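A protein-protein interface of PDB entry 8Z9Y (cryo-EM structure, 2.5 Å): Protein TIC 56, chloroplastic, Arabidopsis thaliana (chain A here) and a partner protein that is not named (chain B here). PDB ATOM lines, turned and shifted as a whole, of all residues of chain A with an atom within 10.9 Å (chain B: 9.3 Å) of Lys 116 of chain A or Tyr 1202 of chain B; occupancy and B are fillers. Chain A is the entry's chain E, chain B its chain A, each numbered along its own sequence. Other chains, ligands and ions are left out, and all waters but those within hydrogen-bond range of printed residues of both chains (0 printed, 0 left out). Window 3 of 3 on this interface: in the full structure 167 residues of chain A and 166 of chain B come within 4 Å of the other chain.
The side-chain amide oxygen (OD1) of Asn 1178 of chain B lies close to the guanidinium group (NE) of Arg 122 of chain A, 3.3 Å away.
NZ of Lys 1191 of chain B is in salt-bridge range of OE1 of Glu 114 of chain A, at 3.0 Å.
The backbone carbonyl oxygen (O) of Phe 1200 of chain B lies within hydrogen-bond range of the backbone NH (N) of Gln 1195 of chain B, 3.4 Å away.
The side-chain hydroxyl (OG) of Ser 120 of chain A is in hydrogen-bond range of the backbone carbonyl oxygen (O) of Lys 116 of chain A, at 3.5 Å.
The side-chain hydroxyl (OG) of Ser 120 of chain A lies within hydrogen-bond range of the backbone carbonyl oxygen (O) of Trp 117 of chain A (2.9 Å).
O of Trp 118 of chain A lies within hydrogen-bond range of NE of Arg 122 of chain A, 2.9 Å away.
The guanidinium group (NH2) of Arg 122 of chain A is in salt-bridge range of the side-chain carboxylate (OE2) of Glu 119 of chain A (3.4 Å).
The backbone carbonyl oxygen (O) of Phe 121 of chain A sits at hydrogen-bond distance from the side-chain hydroxyl (OG) of Ser 124 of chain A, at 3.4 Å.
NE2 of Gln 115 of chain A touches CG2 of Ile 1181 of chain B, 3.7 Å away.
NZ of Lys 116 of chain A touches CE2 of Tyr 1202 of chain B, 3.2 Å away.
Lys 1191 of chain B touches Trp 117 of chain A (CE to NE1, 3.4 Å).
Asn 1178 of chain B touches Trp 118 of chain A (ND2 to CD2, 3.3 Å).
Ser 120 of chain A touches Phe 1200 of chain B (OG to CZ, 3.1 Å).
Phe 121 of chain A touches Phe 1200 of chain B.
No residue of chain B comes within 4 Å of Ala 113 of chain A.
Of the printed residues of chain B, Trp 117 of chain A touches Lys 1191.
Of the printed residues of chain B, Trp 118 of chain A touches Asn 1178 (3.3 Å).
Of the printed residues of chain A, Asn 1178 of chain B touches Trp 118 and Arg 122.
Of the printed residues of chain A, Ile 1181 of chain B touches Gln 115.
Printed residues of chain A within 4 Å of Phe 1200 of chain B: Ser 120 (3.1 Å) and Phe 121 (3.5 Å).
No residue of chain A comes within 4 Å of His 1201 of chain B.
Printed residues of chain A within 4 Å of Tyr 1202 of chain B: Lys 116.
The nearest residue of chain B that does not touch Lys 116 of chain A is Phe 1200 of chain B (6.6 Å).
Of the 17 printed residues of chain A, 8 touch a printed residue of chain B.
Among the printed residues, 8 pairs touch across the chains.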
ATOM      1  N   THR A 108      27.635  -1.966 -14.363  1.00  0.00           N
ATOM      2  CA  THR A 108      26.939  -1.118 -15.325  1.00  0.00           C
ATOM      3  C   THR A 108      25.464  -1.474 -15.463  1.00  0.00           C
ATOM      4  O   THR A 108      24.649  -0.599 -15.786  1.00  0.00           O
ATOM      5  CB  THR A 108      27.620  -1.206 -16.692  1.00  0.00           C
ATOM      6  OG1 THR A 108      27.077  -2.311 -17.427  1.00  0.00           O
ATOM      7  CG2 THR A 108      29.120  -1.401 -16.529  1.00  0.00           C
ATOM      8  N   GLU A 109      25.104  -2.740 -15.245  1.00  0.00           N
ATOM      9  CA  GLU A 109      23.718  -3.150 -15.447  1.00  0.00           C
ATOM     10  C   GLU A 109      22.783  -2.441 -14.475  1.00  0.00           C
ATOM     11  O   GLU A 109      21.688  -2.017 -14.858  1.00  0.00           O
ATOM     12  CB  GLU A 109      23.589  -4.672 -15.330  1.00  0.00           C
ATOM     13  CG  GLU A 109      23.759  -5.243 -13.931  1.00  0.00           C
ATOM     14  CD  GLU A 109      25.202  -5.566 -13.607  1.00  0.00           C
ATOM     15  OE1 GLU A 109      26.058  -5.423 -14.505  1.00  0.00           O
ATOM     16  OE2 GLU A 109      25.481  -5.963 -12.456  1.00  0.00           O
ATOM     17  N   GLU A 110      23.206  -2.271 -13.221  1.00  0.00           N
ATOM     18  CA  GLU A 110      22.334  -1.635 -12.238  1.00  0.00           C
ATOM     19  C   GLU A 110      22.133  -0.155 -12.542  1.00  0.00           C
ATOM     20  O   GLU A 110      21.009   0.354 -12.455  1.00  0.00           O
ATOM     21  CB  GLU A 110      22.900  -1.826 -10.833  1.00  0.00           C
ATOM     22  CG  GLU A 110      21.838  -1.872  -9.749  1.00  0.00           C
ATOM     23  CD  GLU A 110      20.668  -2.763 -10.116  1.00  0.00           C
ATOM     24  OE1 GLU A 110      20.897  -3.950 -10.430  1.00  0.00           O
ATOM     25  OE2 GLU A 110      19.519  -2.275 -10.090  1.00  0.00           O
ATOM     26  N   ILE A 111      23.205   0.553 -12.907  1.00  0.00           N
ATOM     27  CA  ILE A 111      23.069   1.976 -13.194  1.00  0.00           C
ATOM     28  C   ILE A 111      22.257   2.193 -14.467  1.00  0.00           C
ATOM     29  O   ILE A 111      21.432   3.112 -14.539  1.00  0.00           O
ATOM     30  CB  ILE A 111      24.450   2.660 -13.260  1.00  0.00           C
ATOM     31  CG1 ILE A 111      24.315   4.104 -13.749  1.00  0.00           C
ATOM     32  CG2 ILE A 111      25.403   1.888 -14.141  1.00  0.00           C
ATOM     33  CD1 ILE A 111      25.620   4.868 -13.765  1.00  0.00           C
ATOM     34  N   GLU A 112      22.447   1.343 -15.484  1.00  0.00           N
ATOM     35  CA  GLU A 112      21.631   1.489 -16.686  1.00  0.00           C
ATOM     36  C   GLU A 112      20.171   1.130 -16.420  1.00  0.00           C
ATOM     37  O   GLU A 112      19.267   1.755 -16.993  1.00  0.00           O
ATOM     38  CB  GLU A 112      22.213   0.650 -17.831  1.00  0.00           C
ATOM     39  CG  GLU A 112      21.953  -0.846 -17.753  1.00  0.00           C
ATOM     40  CD  GLU A 112      20.697  -1.262 -18.495  1.00  0.00           C
ATOM     41  OE1 GLU A 112      20.494  -0.788 -19.633  1.00  0.00           O
ATOM     42  OE2 GLU A 112      19.914  -2.059 -17.940  1.00  0.00           O
ATOM     43  N   ALA A 113      19.917   0.148 -15.550  1.00  0.00           N
ATOM     44  CA  ALA A 113      18.546  -0.170 -15.171  1.00  0.00           C
ATOM     45  C   ALA A 113      17.897   0.998 -14.444  1.00  0.00           C
ATOM     46  O   ALA A 113      16.729   1.320 -14.688  1.00  0.00           O
ATOM     47  CB  ALA A 113      18.518  -1.427 -14.302  1.00  0.00           C
ATOM     48  N   GLU A 114      18.638   1.651 -13.549  1.00  0.00           N
ATOM     49  CA  GLU A 114      18.091   2.820 -12.871  1.00  0.00           C
ATOM     50  C   GLU A 114      17.848   3.962 -13.850  1.00  0.00           C
ATOM     51  O   GLU A 114      16.857   4.690 -13.728  1.00  0.00           O
ATOM     52  CB  GLU A 114      19.020   3.260 -11.741  1.00  0.00           C
ATOM     53  CG  GLU A 114      18.875   2.428 -10.477  1.00  0.00           C
ATOM     54  CD  GLU A 114      17.536   1.715 -10.393  1.00  0.00           C
ATOM     55  OE1 GLU A 114      16.545   2.349  -9.977  1.00  0.00           O
ATOM     56  OE2 GLU A 114      17.476   0.515 -10.736  1.00  0.00           O
ATOM     57  N   GLN A 115      18.736   4.128 -14.833  1.00  0.00           N
ATOM     58  CA  GLN A 115      18.546   5.172 -15.835  1.00  0.00           C
ATOM     59  C   GLN A 115      17.274   4.936 -16.642  1.00  0.00           C
ATOM     60  O   GLN A 115      16.469   5.855 -16.840  1.00  0.00           O
ATOM     61  CB  GLN A 115      19.766   5.241 -16.755  1.00  0.00           C
ATOM     62  CG  GLN A 115      20.685   6.422 -16.487  1.00  0.00           C
ATOM     63  CD  GLN A 115      20.054   7.753 -16.848  1.00  0.00           C
ATOM     64  OE1 GLN A 115      19.067   7.807 -17.582  1.00  0.00           O
ATOM     65  NE2 GLN A 115      20.624   8.837 -16.334  1.00  0.00           N
ATOM     66  N   LYS A 116      17.070   3.701 -17.113  1.00  0.00           N
ATOM     67  CA  LYS A 116      15.861   3.423 -17.884  1.00  0.00           C
ATOM     68  C   LYS A 116      14.613   3.491 -17.012  1.00  0.00           C
ATOM     69  O   LYS A 116      13.551   3.909 -17.489  1.00  0.00           O
ATOM     70  CB  LYS A 116      15.965   2.065 -18.589  1.00  0.00           C
ATOM     71  CG  LYS A 116      16.193   0.867 -17.687  1.00  0.00           C
ATOM     72  CD  LYS A 116      14.894   0.154 -17.340  1.00  0.00           C
ATOM     73  CE  LYS A 116      15.129  -0.943 -16.314  1.00  0.00           C
ATOM     74  NZ  LYS A 116      13.882  -1.335 -15.607  1.00  0.00           N
ATOM     75  N   TRP A 117      14.721   3.107 -15.737  1.00  0.00           N
ATOM     76  CA  TRP A 117      13.595   3.269 -14.824  1.00  0.00           C
ATOM     77  C   TRP A 117      13.230   4.736 -14.661  1.00  0.00           C
ATOM     78  O   TRP A 117      12.047   5.091 -14.664  1.00  0.00           O
ATOM     79  CB  TRP A 117      13.922   2.641 -13.468  1.00  0.00           C
ATOM     80  CG  TRP A 117      12.807   2.742 -12.468  1.00  0.00           C
ATOM     81  CD1 TRP A 117      11.881   1.785 -12.177  1.00  0.00           C
ATOM     82  CD2 TRP A 117      12.515   3.856 -11.613  1.00  0.00           C
ATOM     83  NE1 TRP A 117      11.022   2.236 -11.205  1.00  0.00           N
ATOM     84  CE2 TRP A 117      11.390   3.505 -10.841  1.00  0.00           C
ATOM     85  CE3 TRP A 117      13.091   5.117 -11.430  1.00  0.00           C
ATOM     86  CZ2 TRP A 117      10.832   4.367  -9.901  1.00  0.00           C
ATOM     87  CZ3 TRP A 117      12.534   5.972 -10.499  1.00  0.00           C
ATOM     88  CH2 TRP A 117      11.417   5.594  -9.745  1.00  0.00           C
ATOM     89  N   TRP A 118      14.231   5.606 -14.515  1.00  0.00           N
ATOM     90  CA  TRP A 118      13.957   7.034 -14.399  1.00  0.00           C
ATOM     91  C   TRP A 118      13.331   7.581 -15.676  1.00  0.00           C
ATOM     92  O   TRP A 118      12.397   8.393 -15.622  1.00  0.00           O
ATOM     93  CB  TRP A 118      15.243   7.791 -14.063  1.00  0.00           C
ATOM     94  CG  TRP A 118      15.544   7.836 -12.598  1.00  0.00           C
ATOM     95  CD1 TRP A 118      16.549   7.181 -11.949  1.00  0.00           C
ATOM     96  CD2 TRP A 118      14.832   8.572 -11.596  1.00  0.00           C
ATOM     97  NE1 TRP A 118      16.510   7.466 -10.605  1.00  0.00           N
ATOM     98  CE2 TRP A 118      15.464   8.317 -10.363  1.00  0.00           C
ATOM     99  CE3 TRP A 118      13.723   9.422 -11.623  1.00  0.00           C
ATOM    100  CZ2 TRP A 118      15.024   8.881  -9.169  1.00  0.00           C
ATOM    101  CZ3 TRP A 118      13.288   9.981 -10.435  1.00  0.00           C
ATOM    102  CH2 TRP A 118      13.936   9.708  -9.225  1.00  0.00           C
ATOM    103  N   GLU A 119      13.833   7.148 -16.836  1.00  0.00           N
ATOM    104  CA  GLU A 119      13.262   7.607 -18.100  1.00  0.00           C
ATOM    105  C   GLU A 119      11.805   7.182 -18.237  1.00  0.00           C
ATOM    106  O   GLU A 119      10.960   7.969 -18.678  1.00  0.00           O
ATOM    107  CB  GLU A 119      14.087   7.085 -19.277  1.00  0.00           C
ATOM    108  CG  GLU A 119      15.530   7.567 -19.302  1.00  0.00           C
ATOM    109  CD  GLU A 119      15.669   9.012 -19.753  1.00  0.00           C
ATOM    110  OE1 GLU A 119      14.638   9.658 -20.038  1.00  0.00           O
ATOM    111  OE2 GLU A 119      16.815   9.503 -19.822  1.00  0.00           O
ATOM    112  N   SER A 120      11.491   5.938 -17.867  1.00  0.00           N
ATOM    113  CA  SER A 120      10.105   5.485 -17.924  1.00  0.00           C
ATOM    114  C   SER A 120       9.241   6.173 -16.874  1.00  0.00           C
ATOM    115  O   SER A 120       8.041   6.369 -17.090  1.00  0.00           O
ATOM    116  CB  SER A 120      10.042   3.967 -17.752  1.00  0.00           C
ATOM    117  OG  SER A 120      10.248   3.599 -16.401  1.00  0.00           O
ATOM    118  N   PHE A 121       9.831   6.541 -15.735  1.00  0.00           N
ATOM    119  CA  PHE A 121       9.082   7.220 -14.685  1.00  0.00           C
ATOM    120  C   PHE A 121       8.723   8.643 -15.091  1.00  0.00           C
ATOM    121  O   PHE A 121       7.628   9.126 -14.781  1.00  0.00           O
ATOM    122  CB  PHE A 121       9.894   7.218 -13.391  1.00  0.00           C
ATOM    123  CG  PHE A 121       9.225   7.924 -12.248  1.00  0.00           C
ATOM    124  CD1 PHE A 121       8.113   7.377 -11.633  1.00  0.00           C
ATOM    125  CD2 PHE A 121       9.713   9.132 -11.783  1.00  0.00           C
ATOM    126  CE1 PHE A 121       7.501   8.022 -10.577  1.00  0.00           C
ATOM    127  CE2 PHE A 121       9.104   9.782 -10.729  1.00  0.00           C
ATOM    128  CZ  PHE A 121       7.996   9.226 -10.126  1.00  0.00           C
ATOM    129  N   ARG A 122       9.629   9.330 -15.783  1.00  0.00           N
ATOM    130  CA  ARG A 122       9.390  10.714 -16.169  1.00  0.00           C
ATOM    131  C   ARG A 122       8.591  10.848 -17.459  1.00  0.00           C
ATOM    132  O   ARG A 122       8.379  11.975 -17.919  1.00  0.00           O
ATOM    133  CB  ARG A 122      10.720  11.457 -16.310  1.00  0.00           C
ATOM    134  CG  ARG A 122      11.517  11.535 -15.022  1.00  0.00           C
ATOM    135  CD  ARG A 122      12.938  11.998 -15.278  1.00  0.00           C
ATOM    136  NE  ARG A 122      13.846  10.888 -15.538  1.00  0.00           N
ATOM    137  CZ  ARG A 122      14.718  10.854 -16.537  1.00  0.00           C
ATOM    138  NH1 ARG A 122      14.827  11.857 -17.393  1.00  0.00           N
ATOM    139  NH2 ARG A 122      15.501   9.789 -16.679  1.00  0.00           N
ATOM    140  N   ALA A 123       8.146   9.742 -18.052  1.00  0.00           N
ATOM    141  CA  ALA A 123       7.370   9.784 -19.283  1.00  0.00           C
ATOM    142  C   ALA A 123       5.884   9.526 -19.069  1.00  0.00           C
ATOM    143  O   ALA A 123       5.089   9.802 -19.972  1.00  0.00           O
ATOM    144  CB  ALA A 123       7.920   8.768 -20.292  1.00  0.00           C
ATOM    145  N   SER A 124       5.495   9.006 -17.913  1.00  0.00           N
ATOM    146  CA  SER A 124       4.088   8.720 -17.663  1.00  0.00           C
ATOM    147  C   SER A 124       3.315  10.023 -17.491  1.00  0.00           C
ATOM    148  O   SER A 124       3.755  10.904 -16.744  1.00  0.00           O
ATOM    149  CB  SER A 124       3.934   7.847 -16.422  1.00  0.00           C
ATOM    150  OG  SER A 124       4.322   8.550 -15.257  1.00  0.00           O
ATOM    151  N   ASN B1178      16.471  13.511  -9.468  1.00  0.00           N
ATOM    152  CA  ASN B1178      16.705  12.708 -10.663  1.00  0.00           C
ATOM    153  C   ASN B1178      17.855  13.262 -11.494  1.00  0.00           C
ATOM    154  O   ASN B1178      18.565  12.498 -12.159  1.00  0.00           O
ATOM    155  CB  ASN B1178      15.429  12.639 -11.505  1.00  0.00           C
ATOM    156  CG  ASN B1178      15.708  12.310 -12.958  1.00  0.00           C
ATOM    157  OD1 ASN B1178      15.509  13.143 -13.843  1.00  0.00           O
ATOM    158  ND2 ASN B1178      16.170  11.091 -13.213  1.00  0.00           N
ATOM    159  N   ILE B1181      23.002  13.103 -11.638  1.00  0.00           N
ATOM    160  CA  ILE B1181      22.794  11.666 -11.496  1.00  0.00           C
ATOM    161  C   ILE B1181      24.118  10.941 -11.716  1.00  0.00           C
ATOM    162  O   ILE B1181      25.154  11.579 -11.934  1.00  0.00           O
ATOM    163  CB  ILE B1181      21.704  11.187 -12.476  1.00  0.00           C
ATOM    164  CG1 ILE B1181      21.033   9.898 -11.985  1.00  0.00           C
ATOM    165  CG2 ILE B1181      22.268  11.028 -13.885  1.00  0.00           C
ATOM    166  CD1 ILE B1181      20.241  10.069 -10.711  1.00  0.00           C
ATOM    167  N   ASN B1188      14.341   0.853  -3.160  1.00  0.00           N
ATOM    168  CA  ASN B1188      13.280   0.040  -3.740  1.00  0.00           C
ATOM    169  C   ASN B1188      11.967   0.128  -2.975  1.00  0.00           C
ATOM    170  O   ASN B1188      10.934  -0.298  -3.504  1.00  0.00           O
ATOM    171  CB  ASN B1188      13.733  -1.421  -3.817  1.00  0.00           C
ATOM    172  CG  ASN B1188      12.874  -2.251  -4.748  1.00  0.00           C
ATOM    173  OD1 ASN B1188      12.064  -3.064  -4.304  1.00  0.00           O
ATOM    174  ND2 ASN B1188      13.048  -2.051  -6.049  1.00  0.00           N
ATOM    175  N   LYS B1191       9.461   2.207  -4.722  1.00  0.00           N
ATOM    176  CA  LYS B1191       8.858   1.497  -5.846  1.00  0.00           C
ATOM    177  C   LYS B1191       7.594   0.769  -5.408  1.00  0.00           C
ATOM    178  O   LYS B1191       6.556   0.833  -6.081  1.00  0.00           O
ATOM    179  CB  LYS B1191       9.859   0.510  -6.447  1.00  0.00           C
ATOM    180  CG  LYS B1191      10.622   1.034  -7.649  1.00  0.00           C
ATOM    181  CD  LYS B1191      11.987   1.560  -7.246  1.00  0.00           C
ATOM    182  CE  LYS B1191      12.930   1.593  -8.435  1.00  0.00           C
ATOM    183  NZ  LYS B1191      14.293   2.051  -8.054  1.00  0.00           N
ATOM    184  N   VAL B1192       7.664   0.076  -4.270  1.00  0.00           N
ATOM    185  CA  VAL B1192       6.488  -0.600  -3.730  1.00  0.00           C
ATOM    186  C   VAL B1192       5.419   0.417  -3.360  1.00  0.00           C
ATOM    187  O   VAL B1192       4.223   0.189  -3.576  1.00  0.00           O
ATOM    188  CB  VAL B1192       6.885  -1.473  -2.523  1.00  0.00           C
ATOM    189  CG1 VAL B1192       5.650  -2.038  -1.837  1.00  0.00           C
ATOM    190  CG2 VAL B1192       7.817  -2.592  -2.963  1.00  0.00           C
ATOM    191  N   PHE B1194       4.871   3.382  -4.777  1.00  0.00           N
ATOM    192  CA  PHE B1194       4.256   3.861  -6.010  1.00  0.00           C
ATOM    193  C   PHE B1194       3.335   2.810  -6.615  1.00  0.00           C
ATOM    194  O   PHE B1194       2.239   3.133  -7.087  1.00  0.00           O
ATOM    195  CB  PHE B1194       5.338   4.262  -7.013  1.00  0.00           C
ATOM    196  CG  PHE B1194       6.085   5.508  -6.635  1.00  0.00           C
ATOM    197  CD1 PHE B1194       5.443   6.546  -5.982  1.00  0.00           C
ATOM    198  CD2 PHE B1194       7.429   5.642  -6.934  1.00  0.00           C
ATOM    199  CE1 PHE B1194       6.128   7.693  -5.634  1.00  0.00           C
ATOM    200  CE2 PHE B1194       8.120   6.787  -6.588  1.00  0.00           C
ATOM    201  CZ  PHE B1194       7.468   7.814  -5.937  1.00  0.00           C
ATOM    202  N   GLN B1195       3.766   1.546  -6.619  1.00  0.00           N
ATOM    203  CA  GLN B1195       2.925   0.489  -7.170  1.00  0.00           C
ATOM    204  C   GLN B1195       1.650   0.316  -6.355  1.00  0.00           C
ATOM    205  O   GLN B1195       0.569   0.096  -6.917  1.00  0.00           O
ATOM    206  CB  GLN B1195       3.703  -0.824  -7.238  1.00  0.00           C
ATOM    207  CG  GLN B1195       3.100  -1.846  -8.190  1.00  0.00           C
ATOM    208  CD  GLN B1195       4.099  -2.896  -8.632  1.00  0.00           C
ATOM    209  OE1 GLN B1195       4.471  -2.962  -9.803  1.00  0.00           O
ATOM    210  NE2 GLN B1195       4.541  -3.723  -7.693  1.00  0.00           N
ATOM    211  N   GLU B1196       1.755   0.405  -5.028  1.00  0.00           N
ATOM    212  CA  GLU B1196       0.574   0.283  -4.180  1.00  0.00           C
ATOM    213  C   GLU B1196      -0.393   1.435  -4.411  1.00  0.00           C
ATOM    214  O   GLU B1196      -1.611   1.231  -4.465  1.00  0.00           O
ATOM    215  CB  GLU B1196       0.990   0.220  -2.710  1.00  0.00           C
ATOM    216  CG  GLU B1196       1.500  -1.142  -2.266  1.00  0.00           C
ATOM    217  CD  GLU B1196       0.418  -2.202  -2.281  1.00  0.00           C
ATOM    218  OE1 GLU B1196      -0.748  -1.869  -1.979  1.00  0.00           O
ATOM    219  OE2 GLU B1196       0.733  -3.370  -2.593  1.00  0.00           O
ATOM    220  N   GLY B1198      -0.453   3.238  -7.159  1.00  0.00           N
ATOM    221  CA  GLY B1198      -0.770   3.334  -8.568  1.00  0.00           C
ATOM    222  C   GLY B1198      -0.162   4.510  -9.292  1.00  0.00           C
ATOM    223  O   GLY B1198      -0.530   4.761 -10.446  1.00  0.00           O
ATOM    224  N   ILE B1199       0.752   5.246  -8.656  1.00  0.00           N
ATOM    225  CA  ILE B1199       1.382   6.384  -9.321  1.00  0.00           C
ATOM    226  C   ILE B1199       2.223   5.907 -10.499  1.00  0.00           C
ATOM    227  O   ILE B1199       2.117   6.431 -11.615  1.00  0.00           O
ATOM    228  CB  ILE B1199       2.222   7.195  -8.319  1.00  0.00           C
ATOM    229  CG1 ILE B1199       1.393   7.538  -7.080  1.00  0.00           C
ATOM    230  CG2 ILE B1199       2.757   8.458  -8.974  1.00  0.00           C
ATOM    231  CD1 ILE B1199       0.114   8.287  -7.388  1.00  0.00           C
ATOM    232  N   PHE B1200       3.067   4.905 -10.269  1.00  0.00           N
ATOM    233  CA  PHE B1200       3.893   4.346 -11.328  1.00  0.00           C
ATOM    234  C   PHE B1200       4.324   2.944 -10.924  1.00  0.00           C
ATOM    235  O   PHE B1200       4.396   2.621  -9.735  1.00  0.00           O
ATOM    236  CB  PHE B1200       5.117   5.222 -11.610  1.00  0.00           C
ATOM    237  CG  PHE B1200       5.968   4.728 -12.743  1.00  0.00           C
ATOM    238  CD1 PHE B1200       5.535   4.846 -14.052  1.00  0.00           C
ATOM    239  CD2 PHE B1200       7.196   4.139 -12.499  1.00  0.00           C
ATOM    240  CE1 PHE B1200       6.313   4.390 -15.096  1.00  0.00           C
ATOM    241  CE2 PHE B1200       7.979   3.683 -13.539  1.00  0.00           C
ATOM    242  CZ  PHE B1200       7.536   3.808 -14.840  1.00  0.00           C
ATOM    243  N   HIS B1201       4.609   2.119 -11.929  1.00  0.00           N
ATOM    244  CA  HIS B1201       5.052   0.753 -11.696  1.00  0.00           C
ATOM    245  C   HIS B1201       5.784   0.261 -12.934  1.00  0.00           C
ATOM    246  O   HIS B1201       5.672   0.845 -14.016  1.00  0.00           O
ATOM    247  CB  HIS B1201       3.877  -0.173 -11.369  1.00  0.00           C
ATOM    248  CG  HIS B1201       3.070  -0.564 -12.566  1.00  0.00           C
ATOM    249  ND1 HIS B1201       3.282  -1.742 -13.252  1.00  0.00           N
ATOM    250  CD2 HIS B1201       2.057   0.066 -13.204  1.00  0.00           C
ATOM    251  CE1 HIS B1201       2.430  -1.821 -14.260  1.00  0.00           C
ATOM    252  NE2 HIS B1201       1.676  -0.737 -14.252  1.00  0.00           N
ATOM    253  N   TYR B1202       6.530  -0.823 -12.761  1.00  0.00           N
ATOM    254  CA  TYR B1202       7.229  -1.456 -13.872  1.00  0.00           C
ATOM    255  C   TYR B1202       7.654  -2.875 -13.511  1.00  0.00           C
ATOM    256  O   TYR B1202       8.799  -3.111 -13.125  1.00  0.00           O
ATOM    257  CB  TYR B1202       8.450  -0.633 -14.287  1.00  0.00           C
ATOM    258  CG  TYR B1202       9.064  -1.086 -15.590  1.00  0.00           C
ATOM    259  CD1 TYR B1202       8.263  -1.470 -16.657  1.00  0.00           C
ATOM    260  CD2 TYR B1202      10.441  -1.131 -15.753  1.00  0.00           C
ATOM    261  CE1 TYR B1202       8.817  -1.887 -17.852  1.00  0.00           C
ATOM    262  CE2 TYR B1202      11.003  -1.547 -16.945  1.00  0.00           C
ATOM    263  CZ  TYR B1202      10.187  -1.923 -17.990  1.00  0.00           C
ATOM    264  OH  TYR B1202      10.743  -2.337 -19.179  1.00  0.00           O
ATOM    265  N   VAL B1214      -0.522  -1.247 -19.321  1.00  0.00           N
ATOM    266  CA  VAL B1214      -0.905  -0.106 -20.142  1.00  0.00           C
ATOM    267  C   VAL B1214      -2.092   0.617 -19.519  1.00  0.00           C
ATOM    268  O   VAL B1214      -2.704   0.118 -18.574  1.00  0.00           O
ATOM    269  CB  VAL B1214      -1.226  -0.540 -21.583  1.00  0.00           C
ATOM    270  CG1 VAL B1214      -0.149  -1.478 -22.106  1.00  0.00           C
ATOM    271  CG2 VAL B1214      -2.595  -1.202 -21.645  1.00  0.00           C
ATOM    272  N   GLN B1216      -2.245   3.694 -17.799  1.00  0.00           N
ATOM    273  CA  GLN B1216      -1.917   4.040 -16.422  1.00  0.00           C
ATOM    274  C   GLN B1216      -2.999   4.877 -15.755  1.00  0.00           C
ATOM    275  O   GLN B1216      -3.066   4.907 -14.522  1.00  0.00           O
ATOM    276  CB  GLN B1216      -0.585   4.790 -16.367  1.00  0.00           C
ATOM    277  CG  GLN B1216       0.604   3.995 -16.876  1.00  0.00           C
ATOM    278  CD  GLN B1216       0.778   4.106 -18.376  1.00  0.00           C
ATOM    279  OE1 GLN B1216       0.088   4.882 -19.037  1.00  0.00           O
ATOM    280  NE2 GLN B1216       1.704   3.328 -18.924  1.00  0.00           N
ATOM    281  N   ASN B1219      -5.327   2.517 -13.940  1.00  0.00           N
ATOM    282  CA  ASN B1219      -4.617   1.947 -12.801  1.00  0.00           C
ATOM    283  C   ASN B1219      -4.521   2.951 -11.661  1.00  0.00           C
ATOM    284  O   ASN B1219      -4.675   2.589 -10.489  1.00  0.00           O
ATOM    285  CB  ASN B1219      -3.227   1.482 -13.231  1.00  0.00           C
ATOM    286  CG  ASN B1219      -2.548   0.632 -12.179  1.00  0.00           C
ATOM    287  OD1 ASN B1219      -3.201   0.086 -11.291  1.00  0.00           O
ATOM    288  ND2 ASN B1219      -1.228   0.515 -12.274  1.00  0.00           N
